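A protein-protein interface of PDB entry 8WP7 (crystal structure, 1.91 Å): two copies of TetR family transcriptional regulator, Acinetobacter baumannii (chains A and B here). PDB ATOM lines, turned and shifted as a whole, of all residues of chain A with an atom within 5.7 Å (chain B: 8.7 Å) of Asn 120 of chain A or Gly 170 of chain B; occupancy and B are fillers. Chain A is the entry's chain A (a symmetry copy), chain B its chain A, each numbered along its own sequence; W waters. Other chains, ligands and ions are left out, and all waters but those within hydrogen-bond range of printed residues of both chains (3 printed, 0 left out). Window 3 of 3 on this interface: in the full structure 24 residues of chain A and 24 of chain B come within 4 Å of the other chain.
Water W2 lies within hydrogen-bond range of the backbone carbonyl oxygen of Gly 170 of chain B (2.7 Å), the side-chain amide nitrogen of Gln 172 of chain B (3.2 Å) and the side-chain amide nitrogen of Asn 120 of chain A (3.3 Å). Water W1 lies within hydrogen-bond range of NE2 of Gln 116 of chain A and O of Leu 169 of chain B. Water W3 bridges N of Gln 172 of chain B (3.1 Å) and NE2 of Gln 124 of chain A (3.1 Å).
The side-chain amide nitrogen of Asn 120 of chain A lies within hydrogen-bond range of the backbone carbonyl oxygen of Leu 169 of chain B. The backbone carbonyl oxygen of Gln 172 of chain B sits at hydrogen-bond distance from the side-chain amide nitrogen of Gln 124 of chain A (3.0 Å).
Asn 120 of chain A touches just these residues of chain B: Leu 169, Gly 170 and Leu 171. Of the printed residues of chain A, Gly 170 of chain B touches Asn 120 (3.7 Å). Of the printed residues of chain B, Gln 124 of chain A touches Leu 171 (3.5 Å) and Gln 172 (3.0 Å). Of the printed residues of chain A, Ile 166 of chain B touches Met 123. Of the printed residues of chain A, Leu 169 of chain B touches Gln 116, Tyr 119 and Asn 120. Printed residues of chain A within 4 Å of Gln 172 of chain B: Gln 124 (3.0 Å). The nearest printed residue of chain B that does not touch Tyr 119 of chain A is Leu 171 of chain B (5.6 Å).
Among the printed residues, 8 pairs touch across the chains. Among the printed residues, no Asp or Glu carboxylate lies within 4 Å of a Lys or Arg side-chain nitrogen of the other chain.
No position is printed for both chains. Of the 8 pairs that touch across the chains among the printed residues, none has its exchanged pair printed and touching as well.
NE2 of Gln 116 of chain A touches O of Leu 169 of chain B (3.8 Å). Leu 169 of chain B touches Tyr 119 of chain A (CD2 to CE2, 3.995 Å). Gly 170 of chain B touches Asn 120 of chain A. OD1 of Asn 120 of chain A touches CD2 of Leu 171 of chain B (3.4 Å). Met 123 of chain A touches Ile 166 of chain B (CE to CD1, 3.7 Å). Gln 124 of chain A touches Leu 171 of chain B (NE2 to CB, 3.5 Å).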
ATOM      1  N   ILE A 115     -14.010  -8.738  -0.624  1.00  0.00           N
ATOM      2  CA  ILE A 115     -12.776  -9.127  -1.297  1.00  0.00           C
ATOM      3  C   ILE A 115     -13.002  -9.223  -2.797  1.00  0.00           C
ATOM      4  O   ILE A 115     -12.114  -8.902  -3.596  1.00  0.00           O
ATOM      5  CB  ILE A 115     -12.244 -10.450  -0.713  1.00  0.00           C
ATOM      6  CG1 ILE A 115     -12.008 -10.313   0.794  1.00  0.00           C
ATOM      7  CG2 ILE A 115     -10.963 -10.861  -1.412  1.00  0.00           C
ATOM      8  CD1 ILE A 115     -10.827  -9.448   1.152  1.00  0.00           C
ATOM      9  N   GLN A 116     -14.201  -9.653  -3.202  1.00  0.00           N
ATOM     10  CA  GLN A 116     -14.549  -9.709  -4.619  1.00  0.00           C
ATOM     11  C   GLN A 116     -14.388  -8.343  -5.276  1.00  0.00           C
ATOM     12  O   GLN A 116     -13.768  -8.219  -6.341  1.00  0.00           O
ATOM     13  CB  GLN A 116     -15.985 -10.221  -4.779  1.00  0.00           C
ATOM     14  CG  GLN A 116     -16.356 -10.659  -6.191  1.00  0.00           C
ATOM     15  CD  GLN A 116     -16.916  -9.526  -7.023  1.00  0.00           C
ATOM     16  OE1 GLN A 116     -17.482  -8.569  -6.490  1.00  0.00           O
ATOM     17  NE2 GLN A 116     -16.792  -9.641  -8.343  1.00  0.00           N
ATOM     18  N   LYS A 117     -14.931  -7.299  -4.646  1.00  0.00           N
ATOM     19  CA  LYS A 117     -14.807  -5.955  -5.200  1.00  0.00           C
ATOM     20  C   LYS A 117     -13.366  -5.463  -5.151  1.00  0.00           C
ATOM     21  O   LYS A 117     -12.892  -4.829  -6.101  1.00  0.00           O
ATOM     22  CB  LYS A 117     -15.727  -4.985  -4.455  1.00  0.00           C
ATOM     23  CG  LYS A 117     -17.207  -5.350  -4.534  1.00  0.00           C
ATOM     24  CD  LYS A 117     -18.079  -4.314  -3.829  1.00  0.00           C
ATOM     25  CE  LYS A 117     -18.040  -4.489  -2.323  1.00  0.00           C
ATOM     26  NZ  LYS A 117     -19.011  -3.597  -1.618  1.00  0.00           N
ATOM     27  N   ALA A 118     -12.656  -5.739  -4.054  1.00  0.00           N
ATOM     28  CA  ALA A 118     -11.288  -5.243  -3.918  1.00  0.00           C
ATOM     29  C   ALA A 118     -10.349  -5.937  -4.895  1.00  0.00           C
ATOM     30  O   ALA A 118      -9.431  -5.307  -5.432  1.00  0.00           O
ATOM     31  CB  ALA A 118     -10.798  -5.425  -2.480  1.00  0.00           C
ATOM     32  N   TYR A 119     -10.560  -7.233  -5.136  1.00  0.00           N
ATOM     33  CA  TYR A 119      -9.728  -7.947  -6.103  1.00  0.00           C
ATOM     34  C   TYR A 119      -9.863  -7.347  -7.496  1.00  0.00           C
ATOM     35  O   TYR A 119      -8.868  -7.203  -8.218  1.00  0.00           O
ATOM     36  CB  TYR A 119     -10.095  -9.429  -6.130  1.00  0.00           C
ATOM     37  CG  TYR A 119      -9.152 -10.274  -6.967  1.00  0.00           C
ATOM     38  CD1 TYR A 119      -7.948 -10.733  -6.444  1.00  0.00           C
ATOM     39  CD2 TYR A 119      -9.457 -10.594  -8.281  1.00  0.00           C
ATOM     40  CE1 TYR A 119      -7.079 -11.497  -7.204  1.00  0.00           C
ATOM     41  CE2 TYR A 119      -8.592 -11.361  -9.055  1.00  0.00           C
ATOM     42  CZ  TYR A 119      -7.406 -11.809  -8.508  1.00  0.00           C
ATOM     43  OH  TYR A 119      -6.540 -12.572  -9.267  1.00  0.00           O
ATOM     44  N   ASN A 120     -11.087  -6.993  -7.895  1.00  0.00           N
ATOM     45  CA  ASN A 120     -11.273  -6.388  -9.210  1.00  0.00           C
ATOM     46  C   ASN A 120     -10.650  -5.001  -9.273  1.00  0.00           C
ATOM     47  O   ASN A 120     -10.100  -4.613 -10.309  1.00  0.00           O
ATOM     48  CB  ASN A 120     -12.759  -6.327  -9.561  1.00  0.00           C
ATOM     49  CG  ASN A 120     -13.282  -7.644 -10.076  1.00  0.00           C
ATOM     50  OD1 ASN A 120     -12.529  -8.612 -10.211  1.00  0.00           O
ATOM     51  ND2 ASN A 120     -14.573  -7.693 -10.376  1.00  0.00           N
ATOM     52  N   LEU A 121     -10.730  -4.240  -8.180  1.00  0.00           N
ATOM     53  CA  LEU A 121     -10.076  -2.937  -8.142  1.00  0.00           C
ATOM     54  C   LEU A 121      -8.575  -3.074  -8.350  1.00  0.00           C
ATOM     55  O   LEU A 121      -7.964  -2.287  -9.081  1.00  0.00           O
ATOM     56  CB  LEU A 121     -10.359  -2.245  -6.808  1.00  0.00           C
ATOM     57  CG  LEU A 121     -11.730  -1.592  -6.627  1.00  0.00           C
ATOM     58  CD1 LEU A 121     -11.927  -1.184  -5.173  1.00  0.00           C
ATOM     59  CD2 LEU A 121     -11.885  -0.395  -7.550  1.00  0.00           C
ATOM     60  N   ALA A 122      -7.963  -4.074  -7.712  1.00  0.00           N
ATOM     61  CA  ALA A 122      -6.533  -4.295  -7.878  1.00  0.00           C
ATOM     62  C   ALA A 122      -6.204  -4.776  -9.283  1.00  0.00           C
ATOM     63  O   ALA A 122      -5.134  -4.450  -9.814  1.00  0.00           O
ATOM     64  CB  ALA A 122      -6.036  -5.300  -6.841  1.00  0.00           C
ATOM     65  N   MET A 123      -7.102  -5.556  -9.898  1.00  0.00           N
ATOM     66  CA  MET A 123      -6.880  -5.986 -11.276  1.00  0.00           C
ATOM     67  C   MET A 123      -6.937  -4.797 -12.224  1.00  0.00           C
ATOM     68  O   MET A 123      -6.129  -4.695 -13.154  1.00  0.00           O
ATOM     69  CB  MET A 123      -7.915  -7.042 -11.683  1.00  0.00           C
ATOM     70  CG  MET A 123      -7.665  -8.410 -11.063  1.00  0.00           C
ATOM     71  SD  MET A 123      -6.352  -9.355 -11.864  1.00  0.00           S
ATOM     72  CE  MET A 123      -6.672  -8.977 -13.582  1.00  0.00           C
ATOM     73  N   GLN A 124      -7.877  -3.876 -11.995  1.00  0.00           N
ATOM     74  CA  GLN A 124      -7.955  -2.694 -12.844  1.00  0.00           C
ATOM     75  C   GLN A 124      -6.733  -1.804 -12.658  1.00  0.00           C
ATOM     76  O   GLN A 124      -6.241  -1.204 -13.620  1.00  0.00           O
ATOM     77  CB  GLN A 124      -9.232  -1.908 -12.547  1.00  0.00           C
ATOM     78  CG  GLN A 124     -10.511  -2.668 -12.838  1.00  0.00           C
ATOM     79  CD  GLN A 124     -10.948  -2.582 -14.293  1.00  0.00           C
ATOM     80  OE1 GLN A 124     -10.360  -1.855 -15.097  1.00  0.00           O
ATOM     81  NE2 GLN A 124     -11.997  -3.324 -14.633  1.00  0.00           N
ATOM     82  N   SER A 125      -6.229  -1.704 -11.422  1.00  0.00           N
ATOM     83  CA  SER A 125      -5.021  -0.927 -11.169  1.00  0.00           C
ATOM     84  C   SER A 125      -3.814  -1.551 -11.857  1.00  0.00           C
ATOM     85  O   SER A 125      -2.971  -0.838 -12.414  1.00  0.00           O
ATOM     86  CB  SER A 125      -4.771  -0.817  -9.665  1.00  0.00           C
ATOM     87  OG  SER A 125      -5.716   0.045  -9.053  1.00  0.00           O
ATOM     88  N   GLU B 164     -10.167 -16.409 -20.684  1.00  0.00           N
ATOM     89  CA  GLU B 164     -11.427 -16.868 -20.102  1.00  0.00           C
ATOM     90  C   GLU B 164     -11.464 -16.634 -18.597  1.00  0.00           C
ATOM     91  O   GLU B 164     -12.516 -16.295 -18.039  1.00  0.00           O
ATOM     92  CB  GLU B 164     -11.631 -18.351 -20.398  1.00  0.00           C
ATOM     93  CG  GLU B 164     -11.590 -18.713 -21.864  1.00  0.00           C
ATOM     94  CD  GLU B 164     -11.376 -20.200 -22.067  1.00  0.00           C
ATOM     95  OE1 GLU B 164     -10.897 -20.596 -23.153  1.00  0.00           O
ATOM     96  OE2 GLU B 164     -11.682 -20.970 -21.131  1.00  0.00           O
ATOM     97  N   GLY B 165     -10.336 -16.840 -17.918  1.00  0.00           N
ATOM     98  CA  GLY B 165     -10.296 -16.588 -16.484  1.00  0.00           C
ATOM     99  C   GLY B 165     -10.557 -15.134 -16.140  1.00  0.00           C
ATOM    100  O   GLY B 165     -11.218 -14.829 -15.144  1.00  0.00           O
ATOM    101  N   ILE B 166     -10.046 -14.218 -16.962  1.00  0.00           N
ATOM    102  CA  ILE B 166     -10.248 -12.795 -16.715  1.00  0.00           C
ATOM    103  C   ILE B 166     -11.706 -12.419 -16.952  1.00  0.00           C
ATOM    104  O   ILE B 166     -12.277 -11.592 -16.228  1.00  0.00           O
ATOM    105  CB  ILE B 166      -9.295 -11.969 -17.597  1.00  0.00           C
ATOM    106  CG1 ILE B 166      -7.848 -12.156 -17.141  1.00  0.00           C
ATOM    107  CG2 ILE B 166      -9.616 -10.508 -17.493  1.00  0.00           C
ATOM    108  CD1 ILE B 166      -7.619 -11.797 -15.698  1.00  0.00           C
ATOM    109  N   TYR B 167     -12.331 -13.016 -17.975  1.00  0.00           N
ATOM    110  CA  TYR B 167     -13.750 -12.776 -18.227  1.00  0.00           C
ATOM    111  C   TYR B 167     -14.612 -13.209 -17.053  1.00  0.00           C
ATOM    112  O   TYR B 167     -15.637 -12.577 -16.771  1.00  0.00           O
ATOM    113  CB  TYR B 167     -14.205 -13.523 -19.480  1.00  0.00           C
ATOM    114  CG  TYR B 167     -13.611 -13.004 -20.760  1.00  0.00           C
ATOM    115  CD1 TYR B 167     -13.212 -11.683 -20.880  1.00  0.00           C
ATOM    116  CD2 TYR B 167     -13.442 -13.843 -21.852  1.00  0.00           C
ATOM    117  CE1 TYR B 167     -12.670 -11.211 -22.051  1.00  0.00           C
ATOM    118  CE2 TYR B 167     -12.901 -13.381 -23.024  1.00  0.00           C
ATOM    119  CZ  TYR B 167     -12.517 -12.066 -23.121  1.00  0.00           C
ATOM    120  OH  TYR B 167     -11.971 -11.603 -24.295  1.00  0.00           O
ATOM    121  N   LYS B 168     -14.225 -14.289 -16.369  1.00  0.00           N
ATOM    122  CA  LYS B 168     -14.998 -14.780 -15.238  1.00  0.00           C
ATOM    123  C   LYS B 168     -15.056 -13.782 -14.090  1.00  0.00           C
ATOM    124  O   LYS B 168     -15.935 -13.900 -13.230  1.00  0.00           O
ATOM    125  CB  LYS B 168     -14.418 -16.098 -14.729  1.00  0.00           C
ATOM    126  CG  LYS B 168     -15.471 -17.089 -14.271  1.00  0.00           C
ATOM    127  CD  LYS B 168     -14.849 -18.391 -13.782  1.00  0.00           C
ATOM    128  CE  LYS B 168     -15.495 -18.844 -12.478  1.00  0.00           C
ATOM    129  NZ  LYS B 168     -15.514 -20.331 -12.342  1.00  0.00           N
ATOM    130  N   LEU B 169     -14.148 -12.807 -14.053  1.00  0.00           N
ATOM    131  CA  LEU B 169     -14.099 -11.879 -12.929  1.00  0.00           C
ATOM    132  C   LEU B 169     -15.198 -10.830 -12.978  1.00  0.00           C
ATOM    133  O   LEU B 169     -15.550 -10.276 -11.930  1.00  0.00           O
ATOM    134  CB  LEU B 169     -12.740 -11.174 -12.873  1.00  0.00           C
ATOM    135  CG  LEU B 169     -11.501 -12.051 -12.678  1.00  0.00           C
ATOM    136  CD1 LEU B 169     -10.240 -11.204 -12.784  1.00  0.00           C
ATOM    137  CD2 LEU B 169     -11.538 -12.777 -11.352  1.00  0.00           C
ATOM    138  N   GLY B 170     -15.740 -10.540 -14.159  1.00  0.00           N
ATOM    139  CA  GLY B 170     -16.749  -9.506 -14.283  1.00  0.00           C
ATOM    140  C   GLY B 170     -16.162  -8.121 -14.112  1.00  0.00           C
ATOM    141  O   GLY B 170     -16.711  -7.285 -13.386  1.00  0.00           O
ATOM    142  N   LEU B 171     -15.036  -7.873 -14.772  1.00  0.00           N
ATOM    143  CA  LEU B 171     -14.388  -6.574 -14.732  1.00  0.00           C
ATOM    144  C   LEU B 171     -15.144  -5.569 -15.592  1.00  0.00           C
ATOM    145  O   LEU B 171     -15.787  -5.927 -16.583  1.00  0.00           O
ATOM    146  CB  LEU B 171     -12.943  -6.685 -15.220  1.00  0.00           C
ATOM    147  CG  LEU B 171     -12.034  -7.568 -14.367  1.00  0.00           C
ATOM    148  CD1 LEU B 171     -10.750  -7.904 -15.108  1.00  0.00           C
ATOM    149  CD2 LEU B 171     -11.725  -6.862 -13.061  1.00  0.00           C
ATOM    150  N   GLN B 172     -15.063  -4.301 -15.197  1.00  0.00           N
ATOM    151  CA  GLN B 172     -15.682  -3.225 -15.958  1.00  0.00           C
ATOM    152  C   GLN B 172     -14.833  -2.896 -17.177  1.00  0.00           C
ATOM    153  O   GLN B 172     -13.603  -2.980 -17.138  1.00  0.00           O
ATOM    154  CB  GLN B 172     -15.844  -1.977 -15.087  1.00  0.00           C
ATOM    155  CG  GLN B 172     -16.650  -2.190 -13.813  1.00  0.00           C
ATOM    156  CD  GLN B 172     -18.072  -2.646 -14.080  1.00  0.00           C
ATOM    157  OE1 GLN B 172     -18.898  -1.880 -14.575  1.00  0.00           O
ATOM    158  NE2 GLN B 172     -18.366  -3.897 -13.743  1.00  0.00           N
ATOM    159  N   GLY B 173     -15.496  -2.519 -18.267  1.00  0.00           N
ATOM    160  CA  GLY B 173     -14.780  -2.104 -19.457  1.00  0.00           C
ATOM    161  C   GLY B 173     -13.995  -3.196 -20.145  1.00  0.00           C
ATOM    162  O   GLY B 173     -12.975  -2.911 -20.778  1.00  0.00           O
ATOM    163  N   LEU B 174     -14.436  -4.447 -20.032  1.00  0.00           N
ATOM    164  CA  LEU B 174     -13.817  -5.568 -20.729  1.00  0.00           C
ATOM    165  C   LEU B 174     -14.923  -6.403 -21.358  1.00  0.00           C
ATOM    166  O   LEU B 174     -15.787  -6.925 -20.646  1.00  0.00           O
ATOM    167  CB  LEU B 174     -12.978  -6.421 -19.777  1.00  0.00           C
ATOM    168  CG  LEU B 174     -12.301  -7.634 -20.412  1.00  0.00           C
ATOM    169  CD1 LEU B 174     -11.407  -7.216 -21.572  1.00  0.00           C
ATOM    170  CD2 LEU B 174     -11.523  -8.413 -19.382  1.00  0.00           C
ATOM    171  N   GLU B 176     -16.398  -9.551 -23.338  1.00  0.00           N
ATOM    172  CA  GLU B 176     -16.197 -10.951 -23.706  1.00  0.00           C
ATOM    173  C   GLU B 176     -16.198 -11.145 -25.216  1.00  0.00           C
ATOM    174  O   GLU B 176     -15.577 -12.085 -25.722  1.00  0.00           O
ATOM    175  CB  GLU B 176     -17.295 -11.816 -23.089  1.00  0.00           C
ATOM    176  CG  GLU B 176     -17.327 -11.825 -21.581  1.00  0.00           C
ATOM    177  CD  GLU B 176     -18.015 -13.056 -21.035  1.00  0.00           C
ATOM    178  OE1 GLU B 176     -18.331 -13.969 -21.829  1.00  0.00           O
ATOM    179  OE2 GLU B 176     -18.264 -13.098 -19.815  1.00  0.00           O
HETATM  180  O   HOH W   1     -15.291 -11.592  -9.405  1.00  0.00           O
HETATM  181  O   HOH W   2     -16.115  -5.154 -11.906  1.00  0.00           O
HETATM  182  O   HOH W   3     -14.021  -3.836 -12.283  1.00  0.00           O
